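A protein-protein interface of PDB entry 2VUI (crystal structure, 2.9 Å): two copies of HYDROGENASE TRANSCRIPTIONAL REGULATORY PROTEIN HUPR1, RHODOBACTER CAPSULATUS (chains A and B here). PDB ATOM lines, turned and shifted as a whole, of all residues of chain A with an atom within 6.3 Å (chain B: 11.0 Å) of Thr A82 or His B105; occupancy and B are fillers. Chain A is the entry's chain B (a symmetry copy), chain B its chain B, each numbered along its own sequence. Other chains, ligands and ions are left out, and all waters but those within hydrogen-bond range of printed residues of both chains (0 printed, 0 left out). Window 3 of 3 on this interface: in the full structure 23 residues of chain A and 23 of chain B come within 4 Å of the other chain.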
ATOM      1  N   THR A  79      29.979 -22.524 -34.096  1.00  0.00           N
ATOM      2  CA  THR A  79      29.962 -21.565 -35.195  1.00  0.00           C
ATOM      3  C   THR A  79      30.773 -20.271 -34.985  1.00  0.00           C
ATOM      4  O   THR A  79      30.802 -19.698 -33.883  1.00  0.00           O
ATOM      5  CB  THR A  79      28.503 -21.238 -35.652  1.00  0.00           C
ATOM      6  OG1 THR A  79      28.474 -20.983 -37.069  1.00  0.00           O
ATOM      7  CG2 THR A  79      27.942 -20.041 -34.901  1.00  0.00           C
ATOM      8  N   GLY A  80      31.434 -19.840 -36.065  1.00  0.00           N
ATOM      9  CA  GLY A  80      32.076 -18.538 -36.136  1.00  0.00           C
ATOM     10  C   GLY A  80      31.167 -17.504 -36.785  1.00  0.00           C
ATOM     11  O   GLY A  80      31.384 -16.303 -36.644  1.00  0.00           O
ATOM     12  N   TYR A  81      30.149 -17.975 -37.498  1.00  0.00           N
ATOM     13  CA  TYR A  81      29.139 -17.099 -38.087  1.00  0.00           C
ATOM     14  C   TYR A  81      27.919 -17.021 -37.174  1.00  0.00           C
ATOM     15  O   TYR A  81      26.830 -17.458 -37.540  1.00  0.00           O
ATOM     16  CB  TYR A  81      28.726 -17.622 -39.462  1.00  0.00           C
ATOM     17  CG  TYR A  81      29.896 -18.029 -40.324  1.00  0.00           C
ATOM     18  CD1 TYR A  81      30.536 -19.243 -40.123  1.00  0.00           C
ATOM     19  CD2 TYR A  81      30.367 -17.202 -41.333  1.00  0.00           C
ATOM     20  CE1 TYR A  81      31.609 -19.628 -40.908  1.00  0.00           C
ATOM     21  CE2 TYR A  81      31.444 -17.578 -42.123  1.00  0.00           C
ATOM     22  CZ  TYR A  81      32.059 -18.794 -41.904  1.00  0.00           C
ATOM     23  OH  TYR A  81      33.128 -19.183 -42.676  1.00  0.00           O
ATOM     24  N   THR A  82      28.107 -16.456 -35.988  1.00  0.00           N
ATOM     25  CA  THR A  82      27.103 -16.521 -34.933  1.00  0.00           C
ATOM     26  C   THR A  82      25.947 -15.551 -35.125  1.00  0.00           C
ATOM     27  O   THR A  82      24.987 -15.576 -34.361  1.00  0.00           O
ATOM     28  CB  THR A  82      27.734 -16.218 -33.572  1.00  0.00           C
ATOM     29  OG1 THR A  82      28.288 -14.899 -33.597  1.00  0.00           O
ATOM     30  CG2 THR A  82      28.841 -17.205 -33.266  1.00  0.00           C
ATOM     31  N   ASP A  83      26.031 -14.702 -36.142  1.00  0.00           N
ATOM     32  CA  ASP A  83      25.098 -13.584 -36.278  1.00  0.00           C
ATOM     33  C   ASP A  83      23.789 -13.919 -37.004  1.00  0.00           C
ATOM     34  O   ASP A  83      22.862 -13.111 -37.010  1.00  0.00           O
ATOM     35  CB  ASP A  83      25.790 -12.396 -36.962  1.00  0.00           C
ATOM     36  CG  ASP A  83      25.061 -11.080 -36.735  1.00  0.00           C
ATOM     37  OD1 ASP A  83      24.137 -11.042 -35.895  1.00  0.00           O
ATOM     38  OD2 ASP A  83      25.415 -10.079 -37.395  1.00  0.00           O
ATOM     39  N   SER A  84      23.705 -15.104 -37.602  1.00  0.00           N
ATOM     40  CA  SER A  84      22.542 -15.462 -38.419  1.00  0.00           C
ATOM     41  C   SER A  84      21.380 -16.045 -37.612  1.00  0.00           C
ATOM     42  O   SER A  84      21.572 -16.937 -36.786  1.00  0.00           O
ATOM     43  CB  SER A  84      22.945 -16.434 -39.530  1.00  0.00           C
ATOM     44  OG  SER A  84      23.358 -17.673 -38.989  1.00  0.00           O
ATOM     45  N   ALA A  85      20.176 -15.539 -37.866  1.00  0.00           N
ATOM     46  CA  ALA A  85      18.976 -15.990 -37.159  1.00  0.00           C
ATOM     47  C   ALA A  85      18.437 -17.287 -37.749  1.00  0.00           C
ATOM     48  O   ALA A  85      18.036 -18.196 -37.018  1.00  0.00           O
ATOM     49  CB  ALA A  85      17.905 -14.911 -37.192  1.00  0.00           C
ATOM     50  N   MET A  87      19.944 -19.702 -38.909  1.00  0.00           N
ATOM     51  CA  MET A  87      20.683 -20.749 -38.222  1.00  0.00           C
ATOM     52  C   MET A  87      20.066 -21.072 -36.879  1.00  0.00           C
ATOM     53  O   MET A  87      19.634 -22.194 -36.640  1.00  0.00           O
ATOM     54  CB  MET A  87      22.126 -20.319 -37.999  1.00  0.00           C
ATOM     55  CG  MET A  87      22.850 -21.156 -36.963  1.00  0.00           C
ATOM     56  SD  MET A  87      24.393 -20.390 -36.436  1.00  0.00           S
ATOM     57  CE  MET A  87      25.425 -20.630 -37.881  1.00  0.00           C
ATOM     58  N   MET A  88      20.037 -20.078 -36.001  1.00  0.00           N
ATOM     59  CA  MET A  88      19.558 -20.273 -34.644  1.00  0.00           C
ATOM     60  C   MET A  88      18.202 -20.936 -34.662  1.00  0.00           C
ATOM     61  O   MET A  88      17.936 -21.840 -33.875  1.00  0.00           O
ATOM     62  CB  MET A  88      19.482 -18.937 -33.925  1.00  0.00           C
ATOM     63  CG  MET A  88      20.787 -18.177 -33.971  1.00  0.00           C
ATOM     64  SD  MET A  88      22.118 -19.099 -33.183  1.00  0.00           S
ATOM     65  CE  MET A  88      23.542 -18.158 -33.739  1.00  0.00           C
ATOM     66  N   PHE A  99      25.664 -24.810 -28.261  1.00  0.00           N
ATOM     67  CA  PHE A  99      26.139 -24.167 -29.492  1.00  0.00           C
ATOM     68  C   PHE A  99      27.293 -23.258 -29.083  1.00  0.00           C
ATOM     69  O   PHE A  99      27.121 -22.369 -28.244  1.00  0.00           O
ATOM     70  CB  PHE A  99      25.008 -23.358 -30.149  1.00  0.00           C
ATOM     71  CG  PHE A  99      25.416 -21.977 -30.630  1.00  0.00           C
ATOM     72  CD1 PHE A  99      25.389 -20.882 -29.767  1.00  0.00           C
ATOM     73  CD2 PHE A  99      25.790 -21.771 -31.945  1.00  0.00           C
ATOM     74  CE1 PHE A  99      25.763 -19.617 -30.201  1.00  0.00           C
ATOM     75  CE2 PHE A  99      26.158 -20.507 -32.385  1.00  0.00           C
ATOM     76  CZ  PHE A  99      26.150 -19.429 -31.512  1.00  0.00           C
ATOM     77  N   LEU A 100      28.477 -23.486 -29.623  1.00  0.00           N
ATOM     78  CA  LEU A 100      29.604 -22.695 -29.190  1.00  0.00           C
ATOM     79  C   LEU A 100      29.993 -21.749 -30.290  1.00  0.00           C
ATOM     80  O   LEU A 100      29.802 -22.038 -31.468  1.00  0.00           O
ATOM     81  CB  LEU A 100      30.775 -23.592 -28.825  1.00  0.00           C
ATOM     82  CG  LEU A 100      30.310 -24.883 -28.151  1.00  0.00           C
ATOM     83  CD1 LEU A 100      31.434 -25.915 -28.092  1.00  0.00           C
ATOM     84  CD2 LEU A 100      29.751 -24.594 -26.769  1.00  0.00           C
ATOM     85  N   THR A 101      30.531 -20.604 -29.899  1.00  0.00           N
ATOM     86  CA  THR A 101      31.030 -19.649 -30.866  1.00  0.00           C
ATOM     87  C   THR A 101      32.509 -19.919 -31.026  1.00  0.00           C
ATOM     88  O   THR A 101      33.156 -20.374 -30.081  1.00  0.00           O
ATOM     89  CB  THR A 101      30.819 -18.202 -30.399  1.00  0.00           C
ATOM     90  OG1 THR A 101      31.905 -17.800 -29.553  1.00  0.00           O
ATOM     91  CG2 THR A 101      29.488 -18.071 -29.650  1.00  0.00           C
ATOM     92  N   LYS A 102      33.023 -19.682 -32.231  1.00  0.00           N
ATOM     93  CA  LYS A 102      34.458 -19.722 -32.490  1.00  0.00           C
ATOM     94  C   LYS A 102      34.966 -18.302 -32.354  1.00  0.00           C
ATOM     95  O   LYS A 102      34.355 -17.385 -32.893  1.00  0.00           O
ATOM     96  CB  LYS A 102      34.755 -20.236 -33.903  1.00  0.00           C
ATOM     97  CG  LYS A 102      34.529 -21.726 -34.098  1.00  0.00           C
ATOM     98  CD  LYS A 102      34.784 -22.122 -35.547  1.00  0.00           C
ATOM     99  CE  LYS A 102      34.552 -23.611 -35.771  1.00  0.00           C
ATOM    100  NZ  LYS A 102      34.893 -24.045 -37.159  1.00  0.00           N
ATOM    101  N   SER B  13      28.097  -6.235 -15.005  1.00  0.00           N
ATOM    102  CA  SER B  13      28.078  -7.543 -15.663  1.00  0.00           C
ATOM    103  C   SER B  13      26.840  -8.335 -15.274  1.00  0.00           C
ATOM    104  O   SER B  13      26.368  -9.187 -16.032  1.00  0.00           O
ATOM    105  CB  SER B  13      29.352  -8.351 -15.367  1.00  0.00           C
ATOM    106  OG  SER B  13      29.798  -8.153 -14.039  1.00  0.00           O
ATOM    107  N   ALA B  16      24.629  -6.948 -17.668  1.00  0.00           N
ATOM    108  CA  ALA B  16      24.808  -7.660 -18.935  1.00  0.00           C
ATOM    109  C   ALA B  16      24.232  -9.077 -18.891  1.00  0.00           C
ATOM    110  O   ALA B  16      23.325  -9.440 -19.644  1.00  0.00           O
ATOM    111  CB  ALA B  16      26.303  -7.711 -19.323  1.00  0.00           C
ATOM    112  N   MET B  17      24.776  -9.887 -18.007  1.00  0.00           N
ATOM    113  CA  MET B  17      24.347 -11.245 -17.970  1.00  0.00           C
ATOM    114  C   MET B  17      22.833 -11.344 -17.938  1.00  0.00           C
ATOM    115  O   MET B  17      22.250 -12.228 -18.557  1.00  0.00           O
ATOM    116  CB  MET B  17      25.004 -11.953 -16.811  1.00  0.00           C
ATOM    117  CG  MET B  17      26.487 -12.066 -17.016  1.00  0.00           C
ATOM    118  SD  MET B  17      27.181 -13.286 -15.905  1.00  0.00           S
ATOM    119  CE  MET B  17      27.283 -12.333 -14.383  1.00  0.00           C
ATOM    120  N   LYS B  18      22.186 -10.426 -17.235  1.00  0.00           N
ATOM    121  CA  LYS B  18      20.731 -10.445 -17.184  1.00  0.00           C
ATOM    122  C   LYS B  18      20.184 -10.234 -18.579  1.00  0.00           C
ATOM    123  O   LYS B  18      19.290 -10.948 -19.004  1.00  0.00           O
ATOM    124  CB  LYS B  18      20.189  -9.372 -16.250  1.00  0.00           C
ATOM    125  CG  LYS B  18      18.674  -9.281 -16.243  1.00  0.00           C
ATOM    126  CD  LYS B  18      18.187  -8.611 -14.948  1.00  0.00           C
ATOM    127  CE  LYS B  18      16.693  -8.254 -14.961  1.00  0.00           C
ATOM    128  NZ  LYS B  18      16.375  -7.196 -13.940  1.00  0.00           N
ATOM    129  N   LEU B  19      20.737  -9.248 -19.283  1.00  0.00           N
ATOM    130  CA  LEU B  19      20.283  -8.854 -20.612  1.00  0.00           C
ATOM    131  C   LEU B  19      20.353 -10.030 -21.565  1.00  0.00           C
ATOM    132  O   LEU B  19      19.617 -10.105 -22.544  1.00  0.00           O
ATOM    133  CB  LEU B  19      21.168  -7.730 -21.152  1.00  0.00           C
ATOM    134  CG  LEU B  19      20.699  -6.276 -21.146  1.00  0.00           C
ATOM    135  CD1 LEU B  19      21.543  -5.506 -22.121  1.00  0.00           C
ATOM    136  CD2 LEU B  19      19.238  -6.164 -21.533  1.00  0.00           C
ATOM    137  N   ALA B  20      21.270 -10.939 -21.278  1.00  0.00           N
ATOM    138  CA  ALA B  20      21.442 -12.129 -22.084  1.00  0.00           C
ATOM    139  C   ALA B  20      20.445 -13.231 -21.686  1.00  0.00           C
ATOM    140  O   ALA B  20      20.049 -14.052 -22.520  1.00  0.00           O
ATOM    141  CB  ALA B  20      22.890 -12.633 -21.978  1.00  0.00           C
ATOM    142  N   LEU B  21      20.034 -13.253 -20.422  1.00  0.00           N
ATOM    143  CA  LEU B  21      19.285 -14.394 -19.905  1.00  0.00           C
ATOM    144  C   LEU B  21      17.843 -14.068 -19.564  1.00  0.00           C
ATOM    145  O   LEU B  21      17.006 -14.976 -19.465  1.00  0.00           O
ATOM    146  CB  LEU B  21      19.959 -14.952 -18.652  1.00  0.00           C
ATOM    147  CG  LEU B  21      21.441 -15.250 -18.821  1.00  0.00           C
ATOM    148  CD1 LEU B  21      22.117 -15.396 -17.479  1.00  0.00           C
ATOM    149  CD2 LEU B  21      21.632 -16.498 -19.663  1.00  0.00           C
ATOM    150  N   ASP B  24      14.767 -15.631 -20.936  1.00  0.00           N
ATOM    151  CA  ASP B  24      14.589 -17.078 -20.881  1.00  0.00           C
ATOM    152  C   ASP B  24      14.456 -17.623 -19.482  1.00  0.00           C
ATOM    153  O   ASP B  24      13.893 -18.708 -19.271  1.00  0.00           O
ATOM    154  CB  ASP B  24      15.732 -17.796 -21.609  1.00  0.00           C
ATOM    155  CG  ASP B  24      15.645 -17.644 -23.119  1.00  0.00           C
ATOM    156  OD1 ASP B  24      14.517 -17.681 -23.658  1.00  0.00           O
ATOM    157  OD2 ASP B  24      16.695 -17.484 -23.776  1.00  0.00           O
ATOM    158  N   ILE B  49      25.497 -18.510 -11.434  1.00  0.00           N
ATOM    159  CA  ILE B  49      26.748 -18.115 -12.067  1.00  0.00           C
ATOM    160  C   ILE B  49      27.501 -17.050 -11.244  1.00  0.00           C
ATOM    161  O   ILE B  49      26.924 -16.048 -10.836  1.00  0.00           O
ATOM    162  CB  ILE B  49      26.503 -17.674 -13.519  1.00  0.00           C
ATOM    163  CG1 ILE B  49      25.682 -18.743 -14.237  1.00  0.00           C
ATOM    164  CG2 ILE B  49      27.825 -17.382 -14.251  1.00  0.00           C
ATOM    165  CD1 ILE B  49      25.146 -18.268 -15.557  1.00  0.00           C
ATOM    166  N   ILE B  78      32.891 -18.107 -13.780  1.00  0.00           N
ATOM    167  CA  ILE B  78      33.178 -17.285 -14.955  1.00  0.00           C
ATOM    168  C   ILE B  78      34.399 -16.409 -14.734  1.00  0.00           C
ATOM    169  O   ILE B  78      34.433 -15.611 -13.776  1.00  0.00           O
ATOM    170  CB  ILE B  78      32.034 -16.312 -15.258  1.00  0.00           C
ATOM    171  CG1 ILE B  78      31.371 -15.887 -13.949  1.00  0.00           C
ATOM    172  CG2 ILE B  78      31.040 -16.923 -16.239  1.00  0.00           C
ATOM    173  CD1 ILE B  78      30.737 -14.546 -14.020  1.00  0.00           C
ATOM    174  N   LEU B 100      33.311 -20.463 -17.469  1.00  0.00           N
ATOM    175  CA  LEU B 100      33.286 -19.738 -18.717  1.00  0.00           C
ATOM    176  C   LEU B 100      34.353 -18.682 -18.695  1.00  0.00           C
ATOM    177  O   LEU B 100      34.708 -18.165 -17.638  1.00  0.00           O
ATOM    178  CB  LEU B 100      31.921 -19.108 -18.938  1.00  0.00           C
ATOM    179  CG  LEU B 100      30.793 -20.008 -18.434  1.00  0.00           C
ATOM    180  CD1 LEU B 100      29.472 -19.248 -18.347  1.00  0.00           C
ATOM    181  CD2 LEU B 100      30.663 -21.244 -19.307  1.00  0.00           C
ATOM    182  N   THR B 101      34.874 -18.367 -19.870  1.00  0.00           N
ATOM    183  CA  THR B 101      35.845 -17.300 -19.991  1.00  0.00           C
ATOM    184  C   THR B 101      35.080 -16.050 -20.359  1.00  0.00           C
ATOM    185  O   THR B 101      34.038 -16.137 -21.011  1.00  0.00           O
ATOM    186  CB  THR B 101      36.891 -17.601 -21.074  1.00  0.00           C
ATOM    187  OG1 THR B 101      36.394 -17.193 -22.356  1.00  0.00           O
ATOM    188  CG2 THR B 101      37.230 -19.095 -21.089  1.00  0.00           C
ATOM    189  N   LYS B 102      35.572 -14.901 -19.898  1.00  0.00           N
ATOM    190  CA  LYS B 102      35.051 -13.604 -20.315  1.00  0.00           C
ATOM    191  C   LYS B 102      35.916 -13.136 -21.467  1.00  0.00           C
ATOM    192  O   LYS B 102      37.137 -13.214 -21.380  1.00  0.00           O
ATOM    193  CB  LYS B 102      35.124 -12.583 -19.175  1.00  0.00           C
ATOM    194  CG  LYS B 102      34.111 -12.797 -18.064  1.00  0.00           C
ATOM    195  CD  LYS B 102      34.311 -11.775 -16.951  1.00  0.00           C
ATOM    196  CE  LYS B 102      33.313 -11.978 -15.818  1.00  0.00           C
ATOM    197  NZ  LYS B 102      33.420 -10.927 -14.761  1.00  0.00           N
ATOM    198  N   PRO B 103      35.295 -12.605 -22.531  1.00  0.00           N
ATOM    199  CA  PRO B 103      33.880 -12.242 -22.599  1.00  0.00           C
ATOM    200  C   PRO B 103      33.091 -13.325 -23.308  1.00  0.00           C
ATOM    201  O   PRO B 103      33.612 -14.407 -23.578  1.00  0.00           O
ATOM    202  CB  PRO B 103      33.897 -10.976 -23.462  1.00  0.00           C
ATOM    203  CG  PRO B 103      35.333 -10.924 -24.087  1.00  0.00           C
ATOM    204  CD  PRO B 103      35.973 -12.245 -23.783  1.00  0.00           C
ATOM    205  N   TRP B 104      31.845 -13.027 -23.640  1.00  0.00           N
ATOM    206  CA  TRP B 104      30.943 -14.093 -23.993  1.00  0.00           C
ATOM    207  C   TRP B 104      29.798 -13.675 -24.863  1.00  0.00           C
ATOM    208  O   TRP B 104      29.200 -12.625 -24.681  1.00  0.00           O
ATOM    209  CB  TRP B 104      30.382 -14.699 -22.717  1.00  0.00           C
ATOM    210  CG  TRP B 104      30.201 -13.686 -21.590  1.00  0.00           C
ATOM    211  CD1 TRP B 104      31.103 -13.373 -20.601  1.00  0.00           C
ATOM    212  CD2 TRP B 104      29.044 -12.879 -21.339  1.00  0.00           C
ATOM    213  NE1 TRP B 104      30.574 -12.425 -19.757  1.00  0.00           N
ATOM    214  CE2 TRP B 104      29.314 -12.104 -20.189  1.00  0.00           C
ATOM    215  CE3 TRP B 104      27.809 -12.731 -21.981  1.00  0.00           C
ATOM    216  CZ2 TRP B 104      28.396 -11.200 -19.670  1.00  0.00           C
ATOM    217  CZ3 TRP B 104      26.899 -11.835 -21.463  1.00  0.00           C
ATOM    218  CH2 TRP B 104      27.198 -11.079 -20.321  1.00  0.00           C
ATOM    219  N   HIS B 105      29.473 -14.538 -25.805  1.00  0.00           N
ATOM    220  CA  HIS B 105      28.283 -14.341 -26.595  1.00  0.00           C
ATOM    221  C   HIS B 105      27.027 -14.502 -25.744  1.00  0.00           C
ATOM    222  O   HIS B 105      26.855 -15.484 -25.006  1.00  0.00           O
ATOM    223  CB  HIS B 105      28.249 -15.273 -27.803  1.00  0.00           C
ATOM    224  CG  HIS B 105      27.560 -14.685 -28.995  1.00  0.00           C
ATOM    225  ND1 HIS B 105      28.068 -13.606 -29.692  1.00  0.00           N
ATOM    226  CD2 HIS B 105      26.404 -15.018 -29.619  1.00  0.00           C
ATOM    227  CE1 HIS B 105      27.256 -13.303 -30.685  1.00  0.00           C
ATOM    228  NE2 HIS B 105      26.236 -14.142 -30.663  1.00  0.00           N
ATOM    229  N   PRO B 106      26.179 -13.471 -25.810  1.00  0.00           N
ATOM    230  CA  PRO B 106      24.760 -13.360 -25.496  1.00  0.00           C
ATOM    231  C   PRO B 106      24.021 -14.632 -25.783  1.00  0.00           C
ATOM    232  O   PRO B 106      22.980 -14.870 -25.171  1.00  0.00           O
ATOM    233  CB  PRO B 106      24.305 -12.310 -26.505  1.00  0.00           C
ATOM    234  CG  PRO B 106      25.494 -11.346 -26.540  1.00  0.00           C
ATOM    235  CD  PRO B 106      26.733 -12.148 -26.163  1.00  0.00           C
ATOM    236  N   GLU B 107      24.540 -15.412 -26.728  1.00  0.00           N
ATOM    237  CA  GLU B 107      23.890 -16.648 -27.154  1.00  0.00           C
ATOM    238  C   GLU B 107      24.689 -17.879 -26.714  1.00  0.00           C
ATOM    239  O   GLU B 107      24.188 -18.996 -26.765  1.00  0.00           O
ATOM    240  CB  GLU B 107      23.655 -16.651 -28.664  1.00  0.00           C
ATOM    241  CG  GLU B 107      22.516 -17.560 -29.098  1.00  0.00           C
ATOM    242  CD  GLU B 107      21.124 -16.955 -28.889  1.00  0.00           C
ATOM    243  OE1 GLU B 107      20.929 -15.760 -29.197  1.00  0.00           O
ATOM    244  OE2 GLU B 107      20.213 -17.685 -28.438  1.00  0.00           O
ATOM    245  N   GLN B 108      25.920 -17.648 -26.262  1.00  0.00           N
ATOM    246  CA  GLN B 108      26.794 -18.697 -25.765  1.00  0.00           C
ATOM    247  C   GLN B 108      26.602 -18.862 -24.272  1.00  0.00           C
ATOM    248  O   GLN B 108      26.236 -19.966 -23.787  1.00  0.00           O
ATOM    249  CB  GLN B 108      28.247 -18.308 -25.977  1.00  0.00           C
ATOM    250  CG  GLN B 108      29.193 -19.294 -25.324  1.00  0.00           C
ATOM    251  CD  GLN B 108      29.350 -20.534 -26.189  1.00  0.00           C
ATOM    252  OE1 GLN B 108      29.372 -20.426 -27.420  1.00  0.00           O
ATOM    253  NE2 GLN B 108      29.461 -21.709 -25.563  1.00  0.00           N
ATOM    254  N   LEU B 109      26.907 -17.764 -23.555  1.00  0.00           N
ATOM    255  CA  LEU B 109      26.574 -17.600 -22.137  1.00  0.00           C
ATOM    256  C   LEU B 109      25.118 -17.950 -21.919  1.00  0.00           C
ATOM    257  O   LEU B 109      24.780 -18.629 -20.973  1.00  0.00           O
ATOM    258  CB  LEU B 109      26.817 -16.165 -21.714  1.00  0.00           C
ATOM    259  CG  LEU B 109      26.298 -15.689 -20.351  1.00  0.00           C
ATOM    260  CD1 LEU B 109      24.883 -15.092 -20.437  1.00  0.00           C
ATOM    261  CD2 LEU B 109      26.350 -16.823 -19.347  1.00  0.00           C
ATOM    262  N   LEU B 110      24.252 -17.497 -22.814  1.00  0.00           N
ATOM    263  CA  LEU B 110      22.857 -17.920 -22.771  1.00  0.00           C
ATOM    264  C   LEU B 110      22.719 -19.429 -22.789  1.00  0.00           C
ATOM    265  O   LEU B 110      21.784 -19.975 -22.216  1.00  0.00           O
ATOM    266  CB  LEU B 110      22.080 -17.348 -23.953  1.00  0.00           C
ATOM    267  CG  LEU B 110      20.730 -18.006 -24.232  1.00  0.00           C
ATOM    268  CD1 LEU B 110      19.899 -18.123 -22.986  1.00  0.00           C
ATOM    269  CD2 LEU B 110      19.976 -17.229 -25.281  1.00  0.00           C
ATOM    270  N   SER B 111      23.638 -20.107 -23.469  1.00  0.00           N
ATOM    271  CA  SER B 111      23.477 -21.536 -23.717  1.00  0.00           C
ATOM    272  C   SER B 111      23.994 -22.318 -22.537  1.00  0.00           C
ATOM    273  O   SER B 111      23.328 -23.251 -22.045  1.00  0.00           O
ATOM    274  CB  SER B 111      24.217 -21.960 -24.977  1.00  0.00           C
ATOM    275  OG  SER B 111      23.703 -23.193 -25.450  1.00  0.00           O
ATOM    276  N   SER B 112      25.182 -21.934 -22.075  1.00  0.00           N
ATOM    277  CA  SER B 112      25.717 -22.572 -20.889  1.00  0.00           C
ATOM    278  C   SER B 112      24.604 -22.571 -19.841  1.00  0.00           C
ATOM    279  O   SER B 112      24.473 -23.520 -19.079  1.00  0.00           O
ATOM    280  CB  SER B 112      26.980 -21.868 -20.409  1.00  0.00           C
ATOM    281  OG  SER B 112      27.754 -21.437 -21.525  1.00  0.00           O
ATOM    282  N   ALA B 113      23.773 -21.527 -19.858  1.00  0.00           N
ATOM    283  CA  ALA B 113      22.612 -21.401 -18.975  1.00  0.00           C
ATOM    284  C   ALA B 113      21.512 -22.452 -19.225  1.00  0.00           C
ATOM    285  O   ALA B 113      21.094 -23.156 -18.301  1.00  0.00           O
ATOM    286  CB  ALA B 113      22.035 -19.989 -19.071  1.00  0.00           C
ATOM    287  N   ARG B 114      21.032 -22.546 -20.464  1.00  0.00           N
ATOM    288  CA  ARG B 114      19.947 -23.475 -20.796  1.00  0.00           C
ATOM    289  C   ARG B 114      20.382 -24.894 -20.478  1.00  0.00           C
ATOM    290  O   ARG B 114      19.589 -25.730 -20.043  1.00  0.00           O
ATOM    291  CB  ARG B 114      19.554 -23.352 -22.268  1.00  0.00           C
ATOM    292  CG  ARG B 114      18.640 -22.179 -22.584  1.00  0.00           C
ATOM    293  CD  ARG B 114      18.348 -22.115 -24.068  1.00  0.00           C
ATOM    294  NE  ARG B 114      17.440 -21.030 -24.428  1.00  0.00           N
ATOM    295  CZ  ARG B 114      17.334 -20.529 -25.656  1.00  0.00           C
ATOM    296  NH1 ARG B 114      18.091 -21.010 -26.635  1.00  0.00           N
ATOM    297  NH2 ARG B 114      16.482 -19.544 -25.905  1.00  0.00           N
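O of Phe A99 lies close to OE1 of Gln B108, 3.1 Å away. OE1 of Gln B108 sits at hydrogen-bond distance from N of Thr A101, at 2.7 Å.
OG of Ser B112 lies within hydrogen-bond range of O of Gln B108 (3.1 Å). The backbone carbonyl oxygen (O) of Leu A100 is in hydrogen-bond range of the backbone NH (N) of Thr A79 (2.7 Å).
OG1 of Thr A82 touches CE1 of His B105 (3.5 Å). CD1 of Phe A99 touches O of Glu B107 (3.7 Å). Ser B111 touches Phe A99. Gln B108 touches Leu A100. CG2 of Thr A101 touches CB of His B105, at 3.6 Å.
Printed residues of chain B within 4 Å of Thr A82: His B105. His B105 touches just these residues of chain A: Thr A82 (3.5 Å) and Thr A101 (3.6 Å). No residue of chain B comes within 4 Å of Thr A79. No residue of chain B comes within 4 Å of Gly A80. No residue of chain B comes within 4 Å of Asp A83. No residue of chain B comes within 4 Å of Ser A84. Thr A101 touches two residues of chain B. Of the printed residues of chain A, Gln B108 touches Phe A99, Leu A100 and Thr A101. Of the printed residues of chain A, Ser B111 touches Phe A99. Of the printed residues of chain B, Phe A99 touches Glu B107, Gln B108 and Ser B111. Printed residues of chain B within 4 Å of Leu A100: Gln B108. The nearest residue of chain B that does not touch Thr A82 is Glu B107 (5.9 Å). The nearest residue of chain A that does not touch His B105 is Phe A99 (4.7 Å).
Hydrophobic or aromatic side chains of chain A within 4 Å of the printed part of chain B: Phe A99 and Leu A100. Along chain A the printed residues that touch a printed residue of chain B span positions 82 to 101. Hydrophobic or aromatic side chains of chain B within 4 Å of the printed part of chain A: His B105. Along chain B the printed residues that touch a printed residue of chain A span positions 105 to 111.
3 positions are printed for both chains.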
